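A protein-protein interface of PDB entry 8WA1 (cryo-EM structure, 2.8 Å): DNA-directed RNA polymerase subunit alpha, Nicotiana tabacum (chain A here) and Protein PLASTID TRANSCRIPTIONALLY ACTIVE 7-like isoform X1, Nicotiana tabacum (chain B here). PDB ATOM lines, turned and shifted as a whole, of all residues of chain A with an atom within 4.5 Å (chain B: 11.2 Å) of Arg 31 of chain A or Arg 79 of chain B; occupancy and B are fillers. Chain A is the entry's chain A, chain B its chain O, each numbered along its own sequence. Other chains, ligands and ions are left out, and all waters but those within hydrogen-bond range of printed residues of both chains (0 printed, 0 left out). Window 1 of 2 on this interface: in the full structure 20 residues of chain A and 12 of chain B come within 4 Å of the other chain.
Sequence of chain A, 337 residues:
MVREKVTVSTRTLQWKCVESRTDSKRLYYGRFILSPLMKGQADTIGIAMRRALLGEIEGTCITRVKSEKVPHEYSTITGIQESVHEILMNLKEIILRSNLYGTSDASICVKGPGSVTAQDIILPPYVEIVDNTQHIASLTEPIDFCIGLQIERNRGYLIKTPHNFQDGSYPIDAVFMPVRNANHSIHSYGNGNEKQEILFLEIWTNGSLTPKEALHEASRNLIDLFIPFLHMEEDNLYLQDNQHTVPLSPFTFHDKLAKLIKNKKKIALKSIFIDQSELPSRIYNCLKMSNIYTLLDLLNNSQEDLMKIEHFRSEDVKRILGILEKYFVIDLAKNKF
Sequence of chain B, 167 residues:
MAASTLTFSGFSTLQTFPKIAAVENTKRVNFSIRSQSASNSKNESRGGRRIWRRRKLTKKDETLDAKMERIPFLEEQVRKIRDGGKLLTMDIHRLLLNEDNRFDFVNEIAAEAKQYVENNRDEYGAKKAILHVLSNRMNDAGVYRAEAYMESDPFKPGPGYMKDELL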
ATOM      1  N   LYS A  16     -18.050   0.404 -17.280  1.00  0.00           N
ATOM      2  CA  LYS A  16     -18.111   1.844 -17.079  1.00  0.00           C
ATOM      3  C   LYS A  16     -18.470   2.131 -15.629  1.00  0.00           C
ATOM      4  O   LYS A  16     -19.299   1.438 -15.031  1.00  0.00           O
ATOM      5  CB  LYS A  16     -19.129   2.495 -18.025  1.00  0.00           C
ATOM      6  CG  LYS A  16     -19.236   4.005 -17.895  1.00  0.00           C
ATOM      7  CD  LYS A  16     -20.331   4.553 -18.795  1.00  0.00           C
ATOM      8  CE  LYS A  16     -21.680   3.940 -18.452  1.00  0.00           C
ATOM      9  NZ  LYS A  16     -22.768   4.450 -19.330  1.00  0.00           N
ATOM     10  N   CYS A  17     -17.837   3.159 -15.071  1.00  0.00           N
ATOM     11  CA  CYS A  17     -18.105   3.597 -13.704  1.00  0.00           C
ATOM     12  C   CYS A  17     -19.257   4.595 -13.736  1.00  0.00           C
ATOM     13  O   CYS A  17     -19.081   5.744 -14.152  1.00  0.00           O
ATOM     14  CB  CYS A  17     -16.856   4.212 -13.078  1.00  0.00           C
ATOM     15  SG  CYS A  17     -17.073   4.773 -11.373  1.00  0.00           S
ATOM     16  N   VAL A  18     -20.438   4.154 -13.299  1.00  0.00           N
ATOM     17  CA  VAL A  18     -21.624   4.998 -13.402  1.00  0.00           C
ATOM     18  C   VAL A  18     -21.686   5.992 -12.248  1.00  0.00           C
ATOM     19  O   VAL A  18     -22.187   7.112 -12.405  1.00  0.00           O
ATOM     20  CB  VAL A  18     -22.893   4.129 -13.477  1.00  0.00           C
ATOM     21  CG1 VAL A  18     -22.897   3.313 -14.759  1.00  0.00           C
ATOM     22  CG2 VAL A  18     -22.993   3.217 -12.265  1.00  0.00           C
ATOM     23  N   GLU A  19     -21.184   5.609 -11.075  1.00  0.00           N
ATOM     24  CA  GLU A  19     -21.235   6.478  -9.910  1.00  0.00           C
ATOM     25  C   GLU A  19     -19.931   6.368  -9.136  1.00  0.00           C
ATOM     26  O   GLU A  19     -19.331   5.294  -9.049  1.00  0.00           O
ATOM     27  CB  GLU A  19     -22.418   6.135  -8.994  1.00  0.00           C
ATOM     28  CG  GLU A  19     -23.781   6.473  -9.575  1.00  0.00           C
ATOM     29  CD  GLU A  19     -24.904   6.280  -8.576  1.00  0.00           C
ATOM     30  OE1 GLU A  19     -24.619   5.875  -7.430  1.00  0.00           O
ATOM     31  OE2 GLU A  19     -26.072   6.537  -8.935  1.00  0.00           O
ATOM     32  N   TYR A  29     -16.626   5.171  -2.517  1.00  0.00           N
ATOM     33  CA  TYR A  29     -17.720   4.417  -3.110  1.00  0.00           C
ATOM     34  C   TYR A  29     -17.658   4.531  -4.624  1.00  0.00           C
ATOM     35  O   TYR A  29     -17.401   5.606  -5.173  1.00  0.00           O
ATOM     36  CB  TYR A  29     -19.086   4.903  -2.607  1.00  0.00           C
ATOM     37  CG  TYR A  29     -20.260   4.310  -3.357  1.00  0.00           C
ATOM     38  CD1 TYR A  29     -20.656   2.998  -3.139  1.00  0.00           C
ATOM     39  CD2 TYR A  29     -20.973   5.064  -4.279  1.00  0.00           C
ATOM     40  CE1 TYR A  29     -21.727   2.453  -3.819  1.00  0.00           C
ATOM     41  CE2 TYR A  29     -22.045   4.527  -4.965  1.00  0.00           C
ATOM     42  CZ  TYR A  29     -22.418   3.221  -4.730  1.00  0.00           C
ATOM     43  OH  TYR A  29     -23.485   2.676  -5.407  1.00  0.00           O
ATOM     44  N   GLY A  30     -17.894   3.411  -5.290  1.00  0.00           N
ATOM     45  CA  GLY A  30     -17.939   3.386  -6.739  1.00  0.00           C
ATOM     46  C   GLY A  30     -18.848   2.279  -7.222  1.00  0.00           C
ATOM     47  O   GLY A  30     -18.895   1.188  -6.650  1.00  0.00           O
ATOM     48  N   ARG A  31     -19.574   2.571  -8.297  1.00  0.00           N
ATOM     49  CA  ARG A  31     -20.476   1.609  -8.909  1.00  0.00           C
ATOM     50  C   ARG A  31     -20.071   1.405 -10.358  1.00  0.00           C
ATOM     51  O   ARG A  31     -19.805   2.371 -11.080  1.00  0.00           O
ATOM     52  CB  ARG A  31     -21.933   2.074  -8.827  1.00  0.00           C
ATOM     53  CG  ARG A  31     -22.945   0.987  -9.141  1.00  0.00           C
ATOM     54  CD  ARG A  31     -24.353   1.553  -9.215  1.00  0.00           C
ATOM     55  NE  ARG A  31     -25.355   0.505  -9.373  1.00  0.00           N
ATOM     56  CZ  ARG A  31     -26.631   0.731  -9.667  1.00  0.00           C
ATOM     57  NH1 ARG A  31     -27.063   1.971  -9.844  1.00  0.00           N
ATOM     58  NH2 ARG A  31     -27.473  -0.285  -9.791  1.00  0.00           N
ATOM     59  N   PHE A  32     -20.031   0.145 -10.781  1.00  0.00           N
ATOM     60  CA  PHE A  32     -19.559  -0.222 -12.107  1.00  0.00           C
ATOM     61  C   PHE A  32     -20.639  -1.022 -12.821  1.00  0.00           C
ATOM     62  O   PHE A  32     -21.645  -1.419 -12.230  1.00  0.00           O
ATOM     63  CB  PHE A  32     -18.250  -1.017 -12.026  1.00  0.00           C
ATOM     64  CG  PHE A  32     -17.150  -0.291 -11.307  1.00  0.00           C
ATOM     65  CD1 PHE A  32     -16.307   0.567 -11.991  1.00  0.00           C
ATOM     66  CD2 PHE A  32     -16.963  -0.460  -9.945  1.00  0.00           C
ATOM     67  CE1 PHE A  32     -15.296   1.240 -11.333  1.00  0.00           C
ATOM     68  CE2 PHE A  32     -15.953   0.210  -9.281  1.00  0.00           C
ATOM     69  CZ  PHE A  32     -15.119   1.061  -9.976  1.00  0.00           C
ATOM     70  N   SER A 185     -25.577  -6.917  -8.223  1.00  0.00           N
ATOM     71  CA  SER A 185     -26.972  -7.050  -8.611  1.00  0.00           C
ATOM     72  C   SER A 185     -27.040  -7.398 -10.090  1.00  0.00           C
ATOM     73  O   SER A 185     -26.078  -7.208 -10.837  1.00  0.00           O
ATOM     74  CB  SER A 185     -27.770  -5.770  -8.331  1.00  0.00           C
ATOM     75  OG  SER A 185     -27.321  -4.703  -9.148  1.00  0.00           O
ATOM     76  N   PHE A 200     -24.102  -5.042 -11.871  1.00  0.00           N
ATOM     77  CA  PHE A 200     -23.759  -3.813 -11.168  1.00  0.00           C
ATOM     78  C   PHE A 200     -22.930  -4.164  -9.940  1.00  0.00           C
ATOM     79  O   PHE A 200     -23.421  -4.843  -9.032  1.00  0.00           O
ATOM     80  CB  PHE A 200     -25.012  -3.039 -10.763  1.00  0.00           C
ATOM     81  CG  PHE A 200     -25.737  -2.412 -11.917  1.00  0.00           C
ATOM     82  CD1 PHE A 200     -25.397  -1.145 -12.359  1.00  0.00           C
ATOM     83  CD2 PHE A 200     -26.764  -3.086 -12.556  1.00  0.00           C
ATOM     84  CE1 PHE A 200     -26.064  -0.563 -13.419  1.00  0.00           C
ATOM     85  CE2 PHE A 200     -27.434  -2.509 -13.616  1.00  0.00           C
ATOM     86  CZ  PHE A 200     -27.084  -1.246 -14.048  1.00  0.00           C
ATOM     87  N   LEU A 201     -21.685  -3.700  -9.911  1.00  0.00           N
ATOM     88  CA  LEU A 201     -20.768  -3.967  -8.812  1.00  0.00           C
ATOM     89  C   LEU A 201     -20.568  -2.703  -7.989  1.00  0.00           C
ATOM     90  O   LEU A 201     -20.190  -1.658  -8.528  1.00  0.00           O
ATOM     91  CB  LEU A 201     -19.423  -4.479  -9.330  1.00  0.00           C
ATOM     92  CG  LEU A 201     -19.160  -5.976  -9.168  1.00  0.00           C
ATOM     93  CD1 LEU A 201     -17.838  -6.360  -9.813  1.00  0.00           C
ATOM     94  CD2 LEU A 201     -19.171  -6.363  -7.697  1.00  0.00           C
ATOM     95  N   GLU A 202     -20.824  -2.802  -6.688  1.00  0.00           N
ATOM     96  CA  GLU A 202     -20.632  -1.706  -5.748  1.00  0.00           C
ATOM     97  C   GLU A 202     -19.490  -2.053  -4.806  1.00  0.00           C
ATOM     98  O   GLU A 202     -19.505  -3.113  -4.170  1.00  0.00           O
ATOM     99  CB  GLU A 202     -21.913  -1.432  -4.957  1.00  0.00           C
ATOM    100  CG  GLU A 202     -23.014  -0.765  -5.763  1.00  0.00           C
ATOM    101  CD  GLU A 202     -24.350  -0.781  -5.047  1.00  0.00           C
ATOM    102  OE1 GLU A 202     -24.950  -1.870  -4.933  1.00  0.00           O
ATOM    103  OE2 GLU A 202     -24.793   0.291  -4.586  1.00  0.00           O
ATOM    104  N   PRO B  72     -22.387   4.567   6.312  1.00  0.00           N
ATOM    105  CA  PRO B  72     -21.532   4.502   5.114  1.00  0.00           C
ATOM    106  C   PRO B  72     -22.107   3.665   3.985  1.00  0.00           C
ATOM    107  O   PRO B  72     -21.816   3.936   2.812  1.00  0.00           O
ATOM    108  CB  PRO B  72     -20.227   3.888   5.650  1.00  0.00           C
ATOM    109  CG  PRO B  72     -20.344   3.916   7.152  1.00  0.00           C
ATOM    110  CD  PRO B  72     -21.800   3.841   7.447  1.00  0.00           C
ATOM    111  N   PHE B  73     -22.920   2.656   4.295  1.00  0.00           N
ATOM    112  CA  PHE B  73     -23.295   1.621   3.332  1.00  0.00           C
ATOM    113  C   PHE B  73     -24.806   1.676   3.104  1.00  0.00           C
ATOM    114  O   PHE B  73     -25.496   0.655   3.116  1.00  0.00           O
ATOM    115  CB  PHE B  73     -22.847   0.240   3.816  1.00  0.00           C
ATOM    116  CG  PHE B  73     -21.414   0.194   4.265  1.00  0.00           C
ATOM    117  CD1 PHE B  73     -20.389   0.110   3.340  1.00  0.00           C
ATOM    118  CD2 PHE B  73     -21.094   0.238   5.612  1.00  0.00           C
ATOM    119  CE1 PHE B  73     -19.070   0.069   3.750  1.00  0.00           C
ATOM    120  CE2 PHE B  73     -19.778   0.197   6.027  1.00  0.00           C
ATOM    121  CZ  PHE B  73     -18.765   0.113   5.096  1.00  0.00           C
ATOM    122  N   LEU B  74     -25.321   2.888   2.899  1.00  0.00           N
ATOM    123  CA  LEU B  74     -26.741   3.093   2.652  1.00  0.00           C
ATOM    124  C   LEU B  74     -27.024   3.664   1.268  1.00  0.00           C
ATOM    125  O   LEU B  74     -28.074   4.284   1.069  1.00  0.00           O
ATOM    126  CB  LEU B  74     -27.335   4.009   3.725  1.00  0.00           C
ATOM    127  CG  LEU B  74     -28.668   3.552   4.315  1.00  0.00           C
ATOM    128  CD1 LEU B  74     -28.575   2.098   4.742  1.00  0.00           C
ATOM    129  CD2 LEU B  74     -29.051   4.431   5.492  1.00  0.00           C
ATOM    130  N   GLU B  75     -26.118   3.473   0.306  1.00  0.00           N
ATOM    131  CA  GLU B  75     -26.345   4.005  -1.034  1.00  0.00           C
ATOM    132  C   GLU B  75     -27.381   3.179  -1.790  1.00  0.00           C
ATOM    133  O   GLU B  75     -28.353   3.725  -2.330  1.00  0.00           O
ATOM    134  CB  GLU B  75     -25.029   4.051  -1.809  1.00  0.00           C
ATOM    135  CG  GLU B  75     -23.799   4.285  -0.947  1.00  0.00           C
ATOM    136  CD  GLU B  75     -23.786   5.649  -0.284  1.00  0.00           C
ATOM    137  OE1 GLU B  75     -24.423   6.581  -0.817  1.00  0.00           O
ATOM    138  OE2 GLU B  75     -23.138   5.788   0.775  1.00  0.00           O
ATOM    139  N   GLU B  76     -27.190   1.858  -1.833  1.00  0.00           N
ATOM    140  CA  GLU B  76     -28.069   1.006  -2.628  1.00  0.00           C
ATOM    141  C   GLU B  76     -29.485   0.991  -2.068  1.00  0.00           C
ATOM    142  O   GLU B  76     -30.456   0.904  -2.827  1.00  0.00           O
ATOM    143  CB  GLU B  76     -27.496  -0.412  -2.696  1.00  0.00           C
ATOM    144  CG  GLU B  76     -28.089  -1.285  -3.797  1.00  0.00           C
ATOM    145  CD  GLU B  76     -29.396  -1.940  -3.396  1.00  0.00           C
ATOM    146  OE1 GLU B  76     -29.663  -2.044  -2.179  1.00  0.00           O
ATOM    147  OE2 GLU B  76     -30.159  -2.350  -4.295  1.00  0.00           O
ATOM    148  N   GLN B  77     -29.626   1.086  -0.744  1.00  0.00           N
ATOM    149  CA  GLN B  77     -30.957   1.102  -0.146  1.00  0.00           C
ATOM    150  C   GLN B  77     -31.746   2.332  -0.579  1.00  0.00           C
ATOM    151  O   GLN B  77     -32.903   2.221  -0.997  1.00  0.00           O
ATOM    152  CB  GLN B  77     -30.851   1.040   1.376  1.00  0.00           C
ATOM    153  CG  GLN B  77     -32.187   1.156   2.085  1.00  0.00           C
ATOM    154  CD  GLN B  77     -32.050   1.118   3.589  1.00  0.00           C
ATOM    155  OE1 GLN B  77     -31.248   0.359   4.131  1.00  0.00           O
ATOM    156  NE2 GLN B  77     -32.827   1.946   4.274  1.00  0.00           N
ATOM    157  N   VAL B  78     -31.137   3.517  -0.479  1.00  0.00           N
ATOM    158  CA  VAL B  78     -31.817   4.739  -0.903  1.00  0.00           C
ATOM    159  C   VAL B  78     -32.079   4.707  -2.402  1.00  0.00           C
ATOM    160  O   VAL B  78     -33.131   5.159  -2.877  1.00  0.00           O
ATOM    161  CB  VAL B  78     -30.999   5.979  -0.492  1.00  0.00           C
ATOM    162  CG1 VAL B  78     -31.678   7.250  -0.973  1.00  0.00           C
ATOM    163  CG2 VAL B  78     -30.811   6.015   1.015  1.00  0.00           C
ATOM    164  N   ARG B  79     -31.132   4.166  -3.173  1.00  0.00           N
ATOM    165  CA  ARG B  79     -31.328   4.039  -4.613  1.00  0.00           C
ATOM    166  C   ARG B  79     -32.551   3.185  -4.926  1.00  0.00           C
ATOM    167  O   ARG B  79     -33.374   3.541  -5.777  1.00  0.00           O
ATOM    168  CB  ARG B  79     -30.080   3.443  -5.258  1.00  0.00           C
ATOM    169  CG  ARG B  79     -30.102   3.429  -6.774  1.00  0.00           C
ATOM    170  CD  ARG B  79     -29.162   2.369  -7.319  1.00  0.00           C
ATOM    171  NE  ARG B  79     -27.993   2.181  -6.463  1.00  0.00           N
ATOM    172  CZ  ARG B  79     -26.879   2.899  -6.547  1.00  0.00           C
ATOM    173  NH1 ARG B  79     -26.773   3.862  -7.452  1.00  0.00           N
ATOM    174  NH2 ARG B  79     -25.868   2.656  -5.724  1.00  0.00           N
ATOM    175  N   LYS B  80     -32.690   2.052  -4.232  1.00  0.00           N
ATOM    176  CA  LYS B  80     -33.818   1.163  -4.482  1.00  0.00           C
ATOM    177  C   LYS B  80     -35.124   1.781  -4.000  1.00  0.00           C
ATOM    178  O   LYS B  80     -36.177   1.583  -4.617  1.00  0.00           O
ATOM    179  CB  LYS B  80     -33.580  -0.187  -3.807  1.00  0.00           C
ATOM    180  CG  LYS B  80     -34.570  -1.269  -4.209  1.00  0.00           C
ATOM    181  CD  LYS B  80     -34.477  -1.577  -5.695  1.00  0.00           C
ATOM    182  CE  LYS B  80     -33.092  -2.080  -6.072  1.00  0.00           C
ATOM    183  NZ  LYS B  80     -32.973  -2.346  -7.533  1.00  0.00           N
ATOM    184  N   ILE B  81     -35.078   2.533  -2.897  1.00  0.00           N
ATOM    185  CA  ILE B  81     -36.276   3.223  -2.421  1.00  0.00           C
ATOM    186  C   ILE B  81     -36.746   4.240  -3.453  1.00  0.00           C
ATOM    187  O   ILE B  81     -37.947   4.362  -3.725  1.00  0.00           O
ATOM    188  CB  ILE B  81     -36.012   3.882  -1.055  1.00  0.00           C
ATOM    189  CG1 ILE B  81     -35.827   2.818   0.028  1.00  0.00           C
ATOM    190  CG2 ILE B  81     -37.153   4.815  -0.680  1.00  0.00           C
ATOM    191  CD1 ILE B  81     -35.522   3.391   1.394  1.00  0.00           C
ATOM    192  N   ARG B  82     -35.810   4.982  -4.049  1.00  0.00           N
ATOM    193  CA  ARG B  82     -36.187   5.966  -5.059  1.00  0.00           C
ATOM    194  C   ARG B  82     -36.689   5.290  -6.330  1.00  0.00           C
ATOM    195  O   ARG B  82     -37.664   5.741  -6.941  1.00  0.00           O
ATOM    196  CB  ARG B  82     -35.006   6.884  -5.375  1.00  0.00           C
ATOM    197  CG  ARG B  82     -34.545   7.741  -4.212  1.00  0.00           C
ATOM    198  CD  ARG B  82     -33.679   8.892  -4.699  1.00  0.00           C
ATOM    199  NE  ARG B  82     -32.700   8.458  -5.692  1.00  0.00           N
ATOM    200  CZ  ARG B  82     -31.464   8.065  -5.403  1.00  0.00           C
ATOM    201  NH1 ARG B  82     -31.049   8.052  -4.144  1.00  0.00           N
ATOM    202  NH2 ARG B  82     -30.642   7.685  -6.371  1.00  0.00           N
ATOM    203  N   ASP B  83     -36.031   4.206  -6.747  1.00  0.00           N
ATOM    204  CA  ASP B  83     -36.373   3.575  -8.018  1.00  0.00           C
ATOM    205  C   ASP B  83     -37.697   2.823  -7.938  1.00  0.00           C
ATOM    206  O   ASP B  83     -38.485   2.843  -8.891  1.00  0.00           O
ATOM    207  CB  ASP B  83     -35.249   2.635  -8.450  1.00  0.00           C
ATOM    208  CG  ASP B  83     -35.366   2.214  -9.900  1.00  0.00           C
ATOM    209  OD1 ASP B  83     -36.148   2.845 -10.642  1.00  0.00           O
ATOM    210  OD2 ASP B  83     -34.676   1.252 -10.298  1.00  0.00           O
ATOM    211  N   GLY B  84     -37.959   2.148  -6.816  1.00  0.00           N
ATOM    212  CA  GLY B  84     -39.141   1.304  -6.730  1.00  0.00           C
ATOM    213  C   GLY B  84     -40.439   2.086  -6.773  1.00  0.00           C
ATOM    214  O   GLY B  84     -41.379   1.707  -7.475  1.00  0.00           O
ATOM    215  N   GLY B  85     -40.513   3.183  -6.024  1.00  0.00           N
ATOM    216  CA  GLY B  85     -41.723   3.980  -5.993  1.00  0.00           C
ATOM    217  C   GLY B  85     -42.249   4.230  -4.595  1.00  0.00           C
ATOM    218  O   GLY B  85     -43.379   4.698  -4.429  1.00  0.00           O
ATOM    219  N   LYS B  86     -41.438   3.922  -3.580  1.00  0.00           N
ATOM    220  CA  LYS B  86     -41.847   4.194  -2.205  1.00  0.00           C
ATOM    221  C   LYS B  86     -41.925   5.691  -1.933  1.00  0.00           C
ATOM    222  O   LYS B  86     -42.568   6.112  -0.962  1.00  0.00           O
ATOM    223  CB  LYS B  86     -40.882   3.522  -1.228  1.00  0.00           C
ATOM    224  CG  LYS B  86     -40.705   2.033  -1.465  1.00  0.00           C
ATOM    225  CD  LYS B  86     -39.878   1.397  -0.363  1.00  0.00           C
ATOM    226  CE  LYS B  86     -40.589   1.488   0.974  1.00  0.00           C
ATOM    227  NZ  LYS B  86     -41.924   0.830   0.930  1.00  0.00           N
ATOM    228  N   LEU B  87     -41.264   6.502  -2.765  1.00  0.00           N
ATOM    229  CA  LEU B  87     -41.403   7.950  -2.661  1.00  0.00           C
ATOM    230  C   LEU B  87     -42.865   8.363  -2.767  1.00  0.00           C
ATOM    231  O   LEU B  87     -43.309   9.290  -2.078  1.00  0.00           O
ATOM    232  CB  LEU B  87     -40.576   8.637  -3.747  1.00  0.00           C
ATOM    233  CG  LEU B  87     -39.169   8.104  -4.020  1.00  0.00           C
ATOM    234  CD1 LEU B  87     -38.549   8.846  -5.191  1.00  0.00           C
ATOM    235  CD2 LEU B  87     -38.288   8.218  -2.789  1.00  0.00           C
ATOM    236  N   MET B  90     -44.477   7.706   0.609  1.00  0.00           N
ATOM    237  CA  MET B  90     -44.058   8.717   1.575  1.00  0.00           C
ATOM    238  C   MET B  90     -44.766  10.043   1.329  1.00  0.00           C
ATOM    239  O   MET B  90     -45.213  10.704   2.274  1.00  0.00           O
ATOM    240  CB  MET B  90     -42.543   8.902   1.523  1.00  0.00           C
ATOM    241  CG  MET B  90     -41.762   7.621   1.723  1.00  0.00           C
ATOM    242  SD  MET B  90     -39.995   7.896   1.934  1.00  0.00           S
ATOM    243  CE  MET B  90     -39.644   8.896   0.493  1.00  0.00           C
ATOM    244  N   GLU B 151     -39.498   8.023 -14.163  1.00  0.00           N
ATOM    245  CA  GLU B 151     -38.072   7.957 -14.431  1.00  0.00           C
ATOM    246  C   GLU B 151     -37.801   6.871 -15.462  1.00  0.00           C
ATOM    247  O   GLU B 151     -38.537   5.887 -15.567  1.00  0.00           O
ATOM    248  CB  GLU B 151     -37.266   7.681 -13.152  1.00  0.00           C
ATOM    249  CG  GLU B 151     -37.222   8.842 -12.171  1.00  0.00           C
ATOM    250  CD  GLU B 151     -36.312   9.967 -12.630  1.00  0.00           C
ATOM    251  OE1 GLU B 151     -35.491   9.738 -13.543  1.00  0.00           O
ATOM    252  OE2 GLU B 151     -36.417  11.082 -12.078  1.00  0.00           O
ATOM    253  N   SER B 152     -36.729   7.062 -16.225  1.00  0.00           N
ATOM    254  CA  SER B 152     -36.323   6.126 -17.261  1.00  0.00           C
ATOM    255  C   SER B 152     -35.017   5.454 -16.861  1.00  0.00           C
ATOM    256  O   SER B 152     -34.194   6.035 -16.150  1.00  0.00           O
ATOM    257  CB  SER B 152     -36.156   6.828 -18.614  1.00  0.00           C
ATOM    258  OG  SER B 152     -37.360   7.458 -19.012  1.00  0.00           O
ATOM    259  N   ASP B 153     -34.839   4.223 -17.324  1.00  0.00           N
ATOM    260  CA  ASP B 153     -33.636   3.465 -17.007  1.00  0.00           C
ATOM    261  C   ASP B 153     -32.507   3.864 -17.949  1.00  0.00           C
ATOM    262  O   ASP B 153     -32.594   3.588 -19.152  1.00  0.00           O
ATOM    263  CB  ASP B 153     -33.907   1.970 -17.114  1.00  0.00           C
ATOM    264  CG  ASP B 153     -34.999   1.507 -16.172  1.00  0.00           C
ATOM    265  OD1 ASP B 153     -35.540   2.351 -15.426  1.00  0.00           O
ATOM    266  OD2 ASP B 153     -35.320   0.301 -16.179  1.00  0.00           O
ATOM    267  N   PRO B 154     -31.444   4.505 -17.458  1.00  0.00           N
ATOM    268  CA  PRO B 154     -30.345   4.876 -18.363  1.00  0.00           C
ATOM    269  C   PRO B 154     -29.546   3.683 -18.845  1.00  0.00           C
ATOM    270  O   PRO B 154     -28.862   3.780 -19.871  1.00  0.00           O
ATOM    271  CB  PRO B 154     -29.486   5.822 -17.508  1.00  0.00           C
ATOM    272  CG  PRO B 154     -30.349   6.192 -16.329  1.00  0.00           C
ATOM    273  CD  PRO B 154     -31.222   5.005 -16.094  1.00  0.00           C
ATOM    274  N   PHE B 155     -29.610   2.559 -18.137  1.00  0.00           N
ATOM    275  CA  PHE B 155     -28.849   1.368 -18.485  1.00  0.00           C
ATOM    276  C   PHE B 155     -29.611   0.424 -19.405  1.00  0.00           C
ATOM    277  O   PHE B 155     -29.228  -0.744 -19.520  1.00  0.00           O
ATOM    278  CB  PHE B 155     -28.433   0.627 -17.210  1.00  0.00           C
ATOM    279  CG  PHE B 155     -28.054   1.541 -16.080  1.00  0.00           C
ATOM    280  CD1 PHE B 155     -26.850   2.224 -16.098  1.00  0.00           C
ATOM    281  CD2 PHE B 155     -28.904   1.720 -15.002  1.00  0.00           C
ATOM    282  CE1 PHE B 155     -26.500   3.068 -15.060  1.00  0.00           C
ATOM    283  CE2 PHE B 155     -28.560   2.562 -13.961  1.00  0.00           C
ATOM    284  CZ  PHE B 155     -27.356   3.236 -13.991  1.00  0.00           C
ATOM    285  N   LYS B 156     -30.676   0.894 -20.044  1.00  0.00           N
ATOM    286  CA  LYS B 156     -31.428   0.048 -20.956  1.00  0.00           C
ATOM    287  C   LYS B 156     -30.531  -0.399 -22.111  1.00  0.00           C
ATOM    288  O   LYS B 156     -29.761   0.409 -22.646  1.00  0.00           O
ATOM    289  CB  LYS B 156     -32.650   0.797 -21.496  1.00  0.00           C
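The side-chain carboxylate (OE1) of Glu 19 of chain A lies within salt-bridge range of the guanidinium group (NH1) of Arg 79 of chain B (2.9 Å).
The side-chain hydroxyl (OH) of Tyr 29 of chain A lies within hydrogen-bond range of the guanidinium group (NH2) of Arg 79 of chain B (2.4 Å).
The guanidinium group (NH2) of Arg 79 of chain B lies within salt-bridge range of the side-chain carboxylate (OE2) of Glu 202 of chain A (2.8 Å).
NH1 of Arg 31 of chain A lies close to NH1 of Arg 79 of chain B (3.1 Å).
Val 18 of chain A touches Phe 155 of chain B (CG1 to CE1, 3.6 Å).
CG of Glu 75 of chain B touches CE1 of Tyr 29 of chain A, at 3.99 Å.
CZ of Phe 200 of chain A touches CG of Phe 155 of chain B, 3.6 Å away.
Glu 76 of chain B touches Glu 202 of chain A (CB to OE2, 3.4 Å).
The side-chain sulfur of Cys 17 of chain A lies within hydrogen-bond range of the backbone carbonyl oxygen of Glu 19 of chain A (3.3 Å).
N of Arg 31 of chain A is in hydrogen-bond range of O of Glu 19 of chain A, at 2.8 Å.
SG of Cys 17 of chain A sits close to O of Arg 31 of chain A, 3.6 Å away.
N of Ser 185 of chain A sits at hydrogen-bond distance from O of Phe 200 of chain A, 3.1 Å away.
The side-chain hydroxyl (OH) of Tyr 29 of chain A is in hydrogen-bond range of the side-chain carboxylate (OE2) of Glu 202 of chain A (2.8 Å).
The backbone NH (N) of Val 18 of chain A sits at hydrogen-bond distance from the backbone carbonyl oxygen (O) of Arg 31 of chain A, at 2.9 Å.
Hydrophobic or aromatic side chains of chain B within 4 Å of the printed part of chain A: Phe 155.
Of the 12 printed residues of chain A, 6 touch a printed residue of chain B.
Printed residues of chain A that touch a printed residue of chain B: Val 18, Glu 19, Tyr 29, Arg 31, Phe 200 and Glu 202.
Arg 79 of chain B touches four residues of chain A.
No residue of chain B comes within 4 Å of Cys 17 of chain A.
No residue of chain B comes within 4 Å of Ser 185 of chain A.
Of chain B, only Phe 155 comes within 4 Å of Phe 200 of chain A.
Glu 202 of chain A touches two residues of chain B.
Of the printed residues of chain A, Phe 155 of chain B touches Val 18 and Phe 200.
Of the printed residues of chain A, Glu 76 of chain B touches Glu 202 (3.4 Å).
Val 78 of chain B touches none of the printed residues of chain A.
Lys 80 of chain B touches none of the printed residues of chain A.
The nearest printed residue of chain A that does not touch Phe 155 of chain B is Arg 31 of chain A (4.3 Å).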
